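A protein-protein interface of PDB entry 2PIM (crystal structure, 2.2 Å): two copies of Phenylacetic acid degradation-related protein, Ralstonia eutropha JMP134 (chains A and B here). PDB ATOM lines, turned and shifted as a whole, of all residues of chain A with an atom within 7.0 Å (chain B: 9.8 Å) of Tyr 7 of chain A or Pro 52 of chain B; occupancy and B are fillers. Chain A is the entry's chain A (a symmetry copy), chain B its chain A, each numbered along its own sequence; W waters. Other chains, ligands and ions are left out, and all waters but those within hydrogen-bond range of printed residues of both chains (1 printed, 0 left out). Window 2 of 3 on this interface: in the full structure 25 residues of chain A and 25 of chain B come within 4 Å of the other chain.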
ATOM      1  N   ASN A   6     -20.570   0.437 -13.738  1.00  0.00           N
ATOM      2  CA  ASN A   6     -19.144   0.480 -13.223  1.00  0.00           C
ATOM      3  C   ASN A   6     -18.525  -0.912 -13.257  1.00  0.00           C
ATOM      4  O   ASN A   6     -19.055  -1.819 -12.619  1.00  0.00           O
ATOM      5  CB  ASN A   6     -19.136   0.975 -11.759  1.00  0.00           C
ATOM      6  CG  ASN A   6     -17.938   1.793 -11.405  1.00  0.00           C
ATOM      7  OD1 ASN A   6     -17.383   2.476 -12.239  1.00  0.00           O
ATOM      8  ND2 ASN A   6     -17.566   1.781 -10.126  1.00  0.00           N
ATOM      9  N   TYR A   7     -17.425  -1.104 -13.981  1.00  0.00           N
ATOM     10  CA  TYR A   7     -16.736  -2.378 -13.879  1.00  0.00           C
ATOM     11  C   TYR A   7     -16.461  -2.701 -12.405  1.00  0.00           C
ATOM     12  O   TYR A   7     -16.661  -3.817 -11.969  1.00  0.00           O
ATOM     13  CB  TYR A   7     -15.412  -2.410 -14.661  1.00  0.00           C
ATOM     14  CG  TYR A   7     -14.439  -3.462 -14.116  1.00  0.00           C
ATOM     15  CD1 TYR A   7     -14.439  -4.781 -14.600  1.00  0.00           C
ATOM     16  CD2 TYR A   7     -13.538  -3.135 -13.086  1.00  0.00           C
ATOM     17  CE1 TYR A   7     -13.556  -5.745 -14.076  1.00  0.00           C
ATOM     18  CE2 TYR A   7     -12.646  -4.082 -12.557  1.00  0.00           C
ATOM     19  CZ  TYR A   7     -12.664  -5.379 -13.052  1.00  0.00           C
ATOM     20  OH  TYR A   7     -11.778  -6.281 -12.507  1.00  0.00           O
ATOM     21  N   PHE A   8     -15.980  -1.716 -11.658  1.00  0.00           N
ATOM     22  CA  PHE A   8     -15.594  -1.906 -10.250  1.00  0.00           C
ATOM     23  C   PHE A   8     -16.742  -2.456  -9.375  1.00  0.00           C
ATOM     24  O   PHE A   8     -16.538  -3.368  -8.569  1.00  0.00           O
ATOM     25  CB  PHE A   8     -15.138  -0.577  -9.680  1.00  0.00           C
ATOM     26  CG  PHE A   8     -14.934  -0.590  -8.208  1.00  0.00           C
ATOM     27  CD1 PHE A   8     -13.704  -0.946  -7.670  1.00  0.00           C
ATOM     28  CD2 PHE A   8     -15.951  -0.218  -7.351  1.00  0.00           C
ATOM     29  CE1 PHE A   8     -13.514  -0.971  -6.318  1.00  0.00           C
ATOM     30  CE2 PHE A   8     -15.758  -0.229  -5.988  1.00  0.00           C
ATOM     31  CZ  PHE A   8     -14.542  -0.591  -5.473  1.00  0.00           C
ATOM     32  N   SER A   9     -17.931  -1.878  -9.502  1.00  0.00           N
ATOM     33  CA  SER A   9     -19.027  -2.302  -8.639  1.00  0.00           C
ATOM     34  C   SER A   9     -19.585  -3.655  -9.084  1.00  0.00           C
ATOM     35  O   SER A   9     -20.070  -4.408  -8.249  1.00  0.00           O
ATOM     36  CB  SER A   9     -20.123  -1.242  -8.534  1.00  0.00           C
ATOM     37  OG  SER A   9     -20.643  -0.993  -9.805  1.00  0.00           O
ATOM     38  N   ARG A  10     -19.490  -3.969 -10.378  1.00  0.00           N
ATOM     39  CA  ARG A  10     -19.767  -5.327 -10.867  1.00  0.00           C
ATOM     40  C   ARG A  10     -18.814  -6.330 -10.221  1.00  0.00           C
ATOM     41  O   ARG A  10     -19.219  -7.390  -9.756  1.00  0.00           O
ATOM     42  CB  ARG A  10     -19.652  -5.405 -12.396  1.00  0.00           C
ATOM     43  CG  ARG A  10     -20.799  -4.746 -13.120  1.00  0.00           C
ATOM     44  CD  ARG A  10     -20.839  -5.154 -14.574  1.00  0.00           C
ATOM     45  NE  ARG A  10     -19.737  -4.574 -15.343  1.00  0.00           N
ATOM     46  CZ  ARG A  10     -19.748  -3.349 -15.869  1.00  0.00           C
ATOM     47  NH1 ARG A  10     -20.793  -2.548 -15.706  1.00  0.00           N
ATOM     48  NH2 ARG A  10     -18.703  -2.913 -16.557  1.00  0.00           N
ATOM     49  N   MET A  11     -17.542  -5.983 -10.201  1.00  0.00           N
ATOM     50  CA  MET A  11     -16.529  -6.805  -9.553  1.00  0.00           C
ATOM     51  C   MET A  11     -16.831  -7.056  -8.061  1.00  0.00           C
ATOM     52  O   MET A  11     -16.656  -8.163  -7.579  1.00  0.00           O
ATOM     53  CB  MET A  11     -15.165  -6.145  -9.721  1.00  0.00           C
ATOM     54  CG  MET A  11     -13.997  -6.973  -9.225  1.00  0.00           C
ATOM     55  SD  MET A  11     -12.567  -5.823  -8.659  1.00  0.00           S
ATOM     56  CE  MET A  11     -13.155  -5.554  -6.794  1.00  0.00           C
ATOM     57  N   LEU A  12     -17.284  -6.037  -7.342  1.00  0.00           N
ATOM     58  CA  LEU A  12     -17.596  -6.174  -5.916  1.00  0.00           C
ATOM     59  C   LEU A  12     -18.722  -7.125  -5.587  1.00  0.00           C
ATOM     60  O   LEU A  12     -18.738  -7.697  -4.512  1.00  0.00           O
ATOM     61  CB  LEU A  12     -18.015  -4.839  -5.316  1.00  0.00           C
ATOM     62  CG  LEU A  12     -16.936  -3.832  -5.002  1.00  0.00           C
ATOM     63  CD1 LEU A  12     -17.600  -2.651  -4.314  1.00  0.00           C
ATOM     64  CD2 LEU A  12     -15.878  -4.443  -4.132  1.00  0.00           C
ATOM     65  N   GLU A  15     -20.000 -10.099 -10.081  1.00  0.00           N
ATOM     66  CA  GLU A  15     -20.518 -10.197 -11.451  1.00  0.00           C
ATOM     67  C   GLU A  15     -19.492  -9.839 -12.517  1.00  0.00           C
ATOM     68  O   GLU A  15     -19.813  -9.744 -13.708  1.00  0.00           O
ATOM     69  CB  GLU A  15     -21.798  -9.366 -11.602  1.00  0.00           C
ATOM     70  CG  GLU A  15     -22.893  -9.721 -10.585  1.00  0.00           C
ATOM     71  CD  GLU A  15     -23.489 -11.137 -10.764  1.00  0.00           C
ATOM     72  OE1 GLU A  15     -22.902 -11.997 -11.473  1.00  0.00           O
ATOM     73  OE2 GLU A  15     -24.585 -11.379 -10.197  1.00  0.00           O
ATOM     74  N   ALA A  16     -18.258  -9.646 -12.063  1.00  0.00           N
ATOM     75  CA  ALA A  16     -17.097  -9.490 -12.922  1.00  0.00           C
ATOM     76  C   ALA A  16     -15.866 -10.031 -12.181  1.00  0.00           C
ATOM     77  O   ALA A  16     -15.826 -10.038 -10.935  1.00  0.00           O
ATOM     78  CB  ALA A  16     -16.885  -8.023 -13.296  1.00  0.00           C
ATOM     79  N   PRO A  17     -14.869 -10.511 -12.954  1.00  0.00           N
ATOM     80  CA  PRO A  17     -13.652 -11.100 -12.380  1.00  0.00           C
ATOM     81  C   PRO A  17     -12.763 -10.094 -11.648  1.00  0.00           C
ATOM     82  O   PRO A  17     -12.518  -8.976 -12.135  1.00  0.00           O
ATOM     83  CB  PRO A  17     -12.930 -11.673 -13.608  1.00  0.00           C
ATOM     84  CG  PRO A  17     -13.420 -10.835 -14.764  1.00  0.00           C
ATOM     85  CD  PRO A  17     -14.852 -10.546 -14.436  1.00  0.00           C
ATOM     86  N   VAL A  18     -12.313 -10.502 -10.466  1.00  0.00           N
ATOM     87  CA  VAL A  18     -11.230  -9.805  -9.784  1.00  0.00           C
ATOM     88  C   VAL A  18      -9.999 -10.022 -10.660  1.00  0.00           C
ATOM     89  O   VAL A  18      -9.833 -11.113 -11.216  1.00  0.00           O
ATOM     90  CB  VAL A  18     -10.974 -10.378  -8.363  1.00  0.00           C
ATOM     91  CG1 VAL A  18      -9.822  -9.646  -7.672  1.00  0.00           C
ATOM     92  CG2 VAL A  18     -12.254 -10.299  -7.511  1.00  0.00           C
ATOM     93  N   PRO A  19      -9.148  -8.990 -10.808  1.00  0.00           N
ATOM     94  CA  PRO A  19      -7.896  -9.183 -11.547  1.00  0.00           C
ATOM     95  C   PRO A  19      -7.048 -10.257 -10.896  1.00  0.00           C
ATOM     96  O   PRO A  19      -6.998 -10.317  -9.675  1.00  0.00           O
ATOM     97  CB  PRO A  19      -7.191  -7.831 -11.428  1.00  0.00           C
ATOM     98  CG  PRO A  19      -8.262  -6.856 -11.033  1.00  0.00           C
ATOM     99  CD  PRO A  19      -9.295  -7.617 -10.299  1.00  0.00           C
ATOM    100  N   ALA A  20      -6.383 -11.083 -11.701  1.00  0.00           N
ATOM    101  CA  ALA A  20      -5.546 -12.147 -11.182  1.00  0.00           C
ATOM    102  C   ALA A  20      -4.530 -11.633 -10.158  1.00  0.00           C
ATOM    103  O   ALA A  20      -4.298 -12.278  -9.135  1.00  0.00           O
ATOM    104  CB  ALA A  20      -4.843 -12.843 -12.303  1.00  0.00           C
ATOM    105  N   VAL A  21      -3.943 -10.468 -10.415  1.00  0.00           N
ATOM    106  CA  VAL A  21      -2.915  -9.930  -9.523  1.00  0.00           C
ATOM    107  C   VAL A  21      -3.458  -9.668  -8.113  1.00  0.00           C
ATOM    108  O   VAL A  21      -2.757  -9.886  -7.128  1.00  0.00           O
ATOM    109  CB  VAL A  21      -2.183  -8.676 -10.135  1.00  0.00           C
ATOM    110  CG1 VAL A  21      -3.144  -7.480 -10.402  1.00  0.00           C
ATOM    111  CG2 VAL A  21      -1.017  -8.249  -9.244  1.00  0.00           C
ATOM    112  N   MET A  71      -7.412   0.853  -7.677  1.00  0.00           N
ATOM    113  CA  MET A  71      -8.793   0.409  -7.385  1.00  0.00           C
ATOM    114  C   MET A  71      -9.670   1.604  -7.055  1.00  0.00           C
ATOM    115  O   MET A  71     -10.805   1.765  -7.580  1.00  0.00           O
ATOM    116  CB  MET A  71      -8.857  -0.603  -6.220  1.00  0.00           C
ATOM    117  CG  MET A  71      -8.657  -2.091  -6.588  1.00  0.00           C
ATOM    118  SD  MET A  71      -9.766  -2.700  -8.106  1.00  0.00           S
ATOM    119  CE  MET A  71      -8.476  -2.314  -9.643  1.00  0.00           C
ATOM    120  N   THR A  74     -10.401   3.537 -10.199  1.00  0.00           N
ATOM    121  CA  THR A  74     -11.373   2.755 -11.013  1.00  0.00           C
ATOM    122  C   THR A  74     -12.789   2.841 -10.487  1.00  0.00           C
ATOM    123  O   THR A  74     -13.761   3.006 -11.257  1.00  0.00           O
ATOM    124  CB  THR A  74     -10.900   1.276 -11.127  1.00  0.00           C
ATOM    125  OG1 THR A  74      -9.610   1.280 -11.730  1.00  0.00           O
ATOM    126  CG2 THR A  74     -11.821   0.440 -11.994  1.00  0.00           C
ATOM    127  N   LEU A  77     -14.765   5.697 -11.984  1.00  0.00           N
ATOM    128  CA  LEU A  77     -14.857   5.854 -13.432  1.00  0.00           C
ATOM    129  C   LEU A  77     -16.198   5.507 -14.019  1.00  0.00           C
ATOM    130  O   LEU A  77     -16.914   4.668 -13.513  1.00  0.00           O
ATOM    131  CB  LEU A  77     -13.761   5.034 -14.121  1.00  0.00           C
ATOM    132  CG  LEU A  77     -12.351   5.409 -13.647  1.00  0.00           C
ATOM    133  CD1 LEU A  77     -11.269   4.820 -14.536  1.00  0.00           C
ATOM    134  CD2 LEU A  77     -12.158   6.925 -13.505  1.00  0.00           C
ATOM    135  N   GLU A  78     -16.543   6.188 -15.099  1.00  0.00           N
ATOM    136  CA  GLU A  78     -17.660   5.772 -15.921  1.00  0.00           C
ATOM    137  C   GLU A  78     -17.298   4.460 -16.630  1.00  0.00           C
ATOM    138  O   GLU A  78     -16.135   4.048 -16.652  1.00  0.00           O
ATOM    139  CB  GLU A  78     -18.042   6.875 -16.926  1.00  0.00           C
ATOM    140  CG  GLU A  78     -16.940   7.295 -17.902  1.00  0.00           C
ATOM    141  CD  GLU A  78     -16.109   8.515 -17.457  1.00  0.00           C
ATOM    142  OE1 GLU A  78     -15.383   8.456 -16.425  1.00  0.00           O
ATOM    143  OE2 GLU A  78     -16.153   9.526 -18.189  1.00  0.00           O
ATOM    144  N   ASP A  79     -18.302   3.792 -17.175  1.00  0.00           N
ATOM    145  CA  ASP A  79     -18.077   2.646 -18.047  1.00  0.00           C
ATOM    146  C   ASP A  79     -17.392   3.130 -19.306  1.00  0.00           C
ATOM    147  O   ASP A  79     -17.795   4.143 -19.889  1.00  0.00           O
ATOM    148  CB  ASP A  79     -19.407   1.969 -18.435  1.00  0.00           C
ATOM    149  CG  ASP A  79     -19.766   0.802 -17.524  1.00  0.00           C
ATOM    150  OD1 ASP A  79     -19.001   0.503 -16.571  1.00  0.00           O
ATOM    151  OD2 ASP A  79     -20.817   0.174 -17.780  1.00  0.00           O
ATOM    152  N   GLY A  80     -16.362   2.407 -19.728  1.00  0.00           N
ATOM    153  CA  GLY A  80     -15.621   2.785 -20.923  1.00  0.00           C
ATOM    154  C   GLY A  80     -14.341   3.536 -20.619  1.00  0.00           C
ATOM    155  O   GLY A  80     -13.381   3.454 -21.394  1.00  0.00           O
ATOM    156  N   ALA A  81     -14.333   4.284 -19.511  1.00  0.00           N
ATOM    157  CA  ALA A  81     -13.127   4.953 -19.024  1.00  0.00           C
ATOM    158  C   ALA A  81     -12.262   3.939 -18.326  1.00  0.00           C
ATOM    159  O   ALA A  81     -12.762   2.926 -17.851  1.00  0.00           O
ATOM    160  CB  ALA A  81     -13.477   6.091 -18.069  1.00  0.00           C
ATOM    161  N   ASP B  47       0.781 -15.473 -15.425  1.00  0.00           N
ATOM    162  CA  ASP B  47      -0.612 -15.070 -15.625  1.00  0.00           C
ATOM    163  C   ASP B  47      -1.208 -14.526 -14.282  1.00  0.00           C
ATOM    164  O   ASP B  47      -2.185 -13.775 -14.272  1.00  0.00           O
ATOM    165  CB  ASP B  47      -1.456 -16.226 -16.181  1.00  0.00           C
ATOM    166  CG  ASP B  47      -1.151 -16.563 -17.665  1.00  0.00           C
ATOM    167  OD1 ASP B  47      -0.630 -15.719 -18.431  1.00  0.00           O
ATOM    168  OD2 ASP B  47      -1.486 -17.703 -18.075  1.00  0.00           O
ATOM    169  N   ALA B  48      -0.566 -14.887 -13.171  1.00  0.00           N
ATOM    170  CA  ALA B  48      -0.967 -14.472 -11.856  1.00  0.00           C
ATOM    171  C   ALA B  48      -0.670 -13.006 -11.557  1.00  0.00           C
ATOM    172  O   ALA B  48      -1.085 -12.489 -10.535  1.00  0.00           O
ATOM    173  CB  ALA B  48      -0.270 -15.340 -10.850  1.00  0.00           C
ATOM    174  N   PHE B  49       0.091 -12.340 -12.414  1.00  0.00           N
ATOM    175  CA  PHE B  49       0.496 -10.978 -12.160  1.00  0.00           C
ATOM    176  C   PHE B  49      -0.260 -10.004 -13.051  1.00  0.00           C
ATOM    177  O   PHE B  49       0.090  -8.826 -13.102  1.00  0.00           O
ATOM    178  CB  PHE B  49       1.985 -10.782 -12.447  1.00  0.00           C
ATOM    179  CG  PHE B  49       2.912 -11.608 -11.617  1.00  0.00           C
ATOM    180  CD1 PHE B  49       2.501 -12.289 -10.491  1.00  0.00           C
ATOM    181  CD2 PHE B  49       4.253 -11.675 -11.987  1.00  0.00           C
ATOM    182  CE1 PHE B  49       3.413 -13.050  -9.753  1.00  0.00           C
ATOM    183  CE2 PHE B  49       5.167 -12.415 -11.265  1.00  0.00           C
ATOM    184  CZ  PHE B  49       4.754 -13.101 -10.152  1.00  0.00           C
ATOM    185  N   LEU B  50      -1.279 -10.501 -13.736  1.00  0.00           N
ATOM    186  CA  LEU B  50      -2.017  -9.752 -14.752  1.00  0.00           C
ATOM    187  C   LEU B  50      -3.221  -8.983 -14.210  1.00  0.00           C
ATOM    188  O   LEU B  50      -3.905  -9.419 -13.265  1.00  0.00           O
ATOM    189  CB  LEU B  50      -2.483 -10.679 -15.880  1.00  0.00           C
ATOM    190  CG  LEU B  50      -1.373 -11.468 -16.584  1.00  0.00           C
ATOM    191  CD1 LEU B  50      -1.938 -12.272 -17.724  1.00  0.00           C
ATOM    192  CD2 LEU B  50      -0.234 -10.577 -17.086  1.00  0.00           C
ATOM    193  N   ASN B  51      -3.413  -7.815 -14.818  1.00  0.00           N
ATOM    194  CA  ASN B  51      -4.598  -6.983 -14.639  1.00  0.00           C
ATOM    195  C   ASN B  51      -5.773  -7.551 -15.467  1.00  0.00           C
ATOM    196  O   ASN B  51      -5.608  -8.533 -16.191  1.00  0.00           O
ATOM    197  CB  ASN B  51      -4.253  -5.506 -14.987  1.00  0.00           C
ATOM    198  CG  ASN B  51      -4.193  -5.225 -16.498  1.00  0.00           C
ATOM    199  OD1 ASN B  51      -4.497  -6.068 -17.328  1.00  0.00           O
ATOM    200  ND2 ASN B  51      -3.793  -4.019 -16.843  1.00  0.00           N
ATOM    201  N   PRO B  52      -6.969  -6.952 -15.362  1.00  0.00           N
ATOM    202  CA  PRO B  52      -8.116  -7.506 -16.106  1.00  0.00           C
ATOM    203  C   PRO B  52      -7.951  -7.588 -17.631  1.00  0.00           C
ATOM    204  O   PRO B  52      -8.515  -8.485 -18.268  1.00  0.00           O
ATOM    205  CB  PRO B  52      -9.251  -6.546 -15.759  1.00  0.00           C
ATOM    206  CG  PRO B  52      -8.860  -5.936 -14.483  1.00  0.00           C
ATOM    207  CD  PRO B  52      -7.367  -5.785 -14.567  1.00  0.00           C
ATOM    208  N   VAL B  53      -7.191  -6.656 -18.203  1.00  0.00           N
ATOM    209  CA  VAL B  53      -6.982  -6.600 -19.655  1.00  0.00           C
ATOM    210  C   VAL B  53      -5.784  -7.463 -20.094  1.00  0.00           C
ATOM    211  O   VAL B  53      -5.428  -7.482 -21.270  1.00  0.00           O
ATOM    212  CB  VAL B  53      -6.884  -5.107 -20.162  1.00  0.00           C
ATOM    213  CG1 VAL B  53      -5.747  -4.334 -19.479  1.00  0.00           C
ATOM    214  CG2 VAL B  53      -6.725  -5.039 -21.672  1.00  0.00           C
ATOM    215  N   GLY B  54      -5.168  -8.192 -19.163  1.00  0.00           N
ATOM    216  CA  GLY B  54      -4.125  -9.152 -19.524  1.00  0.00           C
ATOM    217  C   GLY B  54      -2.716  -8.590 -19.597  1.00  0.00           C
ATOM    218  O   GLY B  54      -1.785  -9.265 -20.059  1.00  0.00           O
ATOM    219  N   GLN B  55      -2.532  -7.360 -19.145  1.00  0.00           N
ATOM    220  CA  GLN B  55      -1.195  -6.828 -19.018  1.00  0.00           C
ATOM    221  C   GLN B  55      -0.670  -6.996 -17.570  1.00  0.00           C
ATOM    222  O   GLN B  55      -1.432  -7.141 -16.613  1.00  0.00           O
ATOM    223  CB  GLN B  55      -1.173  -5.368 -19.431  1.00  0.00           C
ATOM    224  CG  GLN B  55      -1.801  -5.054 -20.781  1.00  0.00           C
ATOM    225  CD  GLN B  55      -2.281  -3.588 -20.843  1.00  0.00           C
ATOM    226  OE1 GLN B  55      -2.029  -2.784 -19.919  1.00  0.00           O
ATOM    227  NE2 GLN B  55      -2.974  -3.237 -21.930  1.00  0.00           N
ATOM    228  N   VAL B  56       0.639  -6.960 -17.424  1.00  0.00           N
ATOM    229  CA  VAL B  56       1.269  -7.127 -16.126  1.00  0.00           C
ATOM    230  C   VAL B  56       0.961  -5.883 -15.274  1.00  0.00           C
ATOM    231  O   VAL B  56       1.157  -4.739 -15.726  1.00  0.00           O
ATOM    232  CB  VAL B  56       2.818  -7.313 -16.257  1.00  0.00           C
ATOM    233  CG1 VAL B  56       3.472  -7.539 -14.910  1.00  0.00           C
ATOM    234  CG2 VAL B  56       3.150  -8.479 -17.153  1.00  0.00           C
ATOM    235  N   GLN B  57       0.512  -6.105 -14.041  1.00  0.00           N
ATOM    236  CA  GLN B  57       0.309  -4.998 -13.100  1.00  0.00           C
ATOM    237  C   GLN B  57       1.615  -4.240 -12.916  1.00  0.00           C
ATOM    238  O   GLN B  57       2.683  -4.873 -12.794  1.00  0.00           O
ATOM    239  CB  GLN B  57      -0.131  -5.513 -11.736  1.00  0.00           C
ATOM    240  CG  GLN B  57      -0.767  -4.437 -10.851  1.00  0.00           C
ATOM    241  CD  GLN B  57      -0.354  -4.560  -9.394  1.00  0.00           C
ATOM    242  OE1 GLN B  57       0.795  -4.909  -9.095  1.00  0.00           O
ATOM    243  NE2 GLN B  57      -1.289  -4.252  -8.472  1.00  0.00           N
ATOM    244  N   GLY B  58       1.512  -2.903 -12.880  1.00  0.00           N
ATOM    245  CA  GLY B  58       2.633  -2.000 -12.715  1.00  0.00           C
ATOM    246  C   GLY B  58       3.434  -2.307 -11.457  1.00  0.00           C
ATOM    247  O   GLY B  58       4.647  -2.361 -11.471  1.00  0.00           O
HETATM  248  O   HOH W   1      -6.816 -10.799 -14.526  1.00  0.00           O
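O of Phe 49 of chain B lies within hydrogen-bond range of N of Gln 57 of chain B, at 2.9 Å. The side-chain hydroxyl (OH) of Tyr 7 of chain A is in hydrogen-bond range of the backbone carbonyl oxygen (O) of Pro 17 of chain A, at 2.8 Å. The backbone NH of Tyr 7 of chain A lies within hydrogen-bond range of the side-chain carboxylate of Asp 79 of chain A, 3.4 Å away.
Pro 52 of chain B touches Tyr 7 of chain A (CG to OH, 3.5 Å). Pro 19 of chain A touches Pro 52 of chain B. CB of Ala 20 of chain A touches O of Asp 47 of chain B (3.4 Å). Ala 20 of chain A touches Ala 48 of chain B. O of Ala 48 of chain B touches CA of Val 21 of chain A, at 3.3 Å. CB of Val 21 of chain A touches C of Phe 49 of chain B, at 3.7 Å. Gln 57 of chain B touches Val 21 of chain A (CD to CG2, 3.8 Å).
N of Ala 20 of chain A lies within hydrogen-bond range of O of Leu 50 of chain B, 3.4 Å away. The backbone carbonyl oxygen (O) of Leu 50 of chain B lies within hydrogen-bond range of the backbone NH (N) of Val 21 of chain A (3.0 Å).
No position is printed for both chains. Of the 9 pairs that touch across the chains among the printed residues, none has its exchanged pair printed and touching as well.
Of the 21 printed residues of chain A, 4 touch a printed residue of chain B. Hydrophobic or aromatic side chains of chain A within 4 Å of the printed part of chain B: Tyr 7, Pro 19, Ala 20 and Val 21. Of the 12 printed residues of chain B, 6 touch a printed residue of chain A. Hydrophobic or aromatic side chains of chain B that line the printed part of chain A: Pro 52. Among the printed residues, no Asp or Glu carboxylate lies within 4 Å of a Lys or Arg side-chain nitrogen of the other chain.
Tyr 7 of chain A touches just one residue of chain B: Pro 52. Ser 9 of chain A touches none of the printed residues of chain B. Of the printed residues of chain B, Val 21 of chain A touches Ala 48, Phe 49, Leu 50 and Gln 57. Of the printed residues of chain A, Phe 49 of chain B touches Val 21 (3.7 Å). Printed residues of chain B within 4 Å of Ala 20 of chain A: Asp 47, Ala 48 and Leu 50. Asn 51 of chain B touches none of the printed residues of chain A. The nearest residue of chain B that does not touch Tyr 7 of chain A is Asn 51 of chain B (6.8 Å). The nearest residue of chain A that does not touch Pro 52 of chain B is Pro 17 of chain A (5.3 Å). The nearest printed residue of chain A that does not touch Asp 47 of chain B is Val 21 of chain A (5.4 Å).
Water W1 lies within hydrogen-bond range of N of Ala 20 of chain A (2.9 Å), O of Asn 51 of chain B (3.1 Å) and O of Leu 50 of chain B (3.5 Å).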
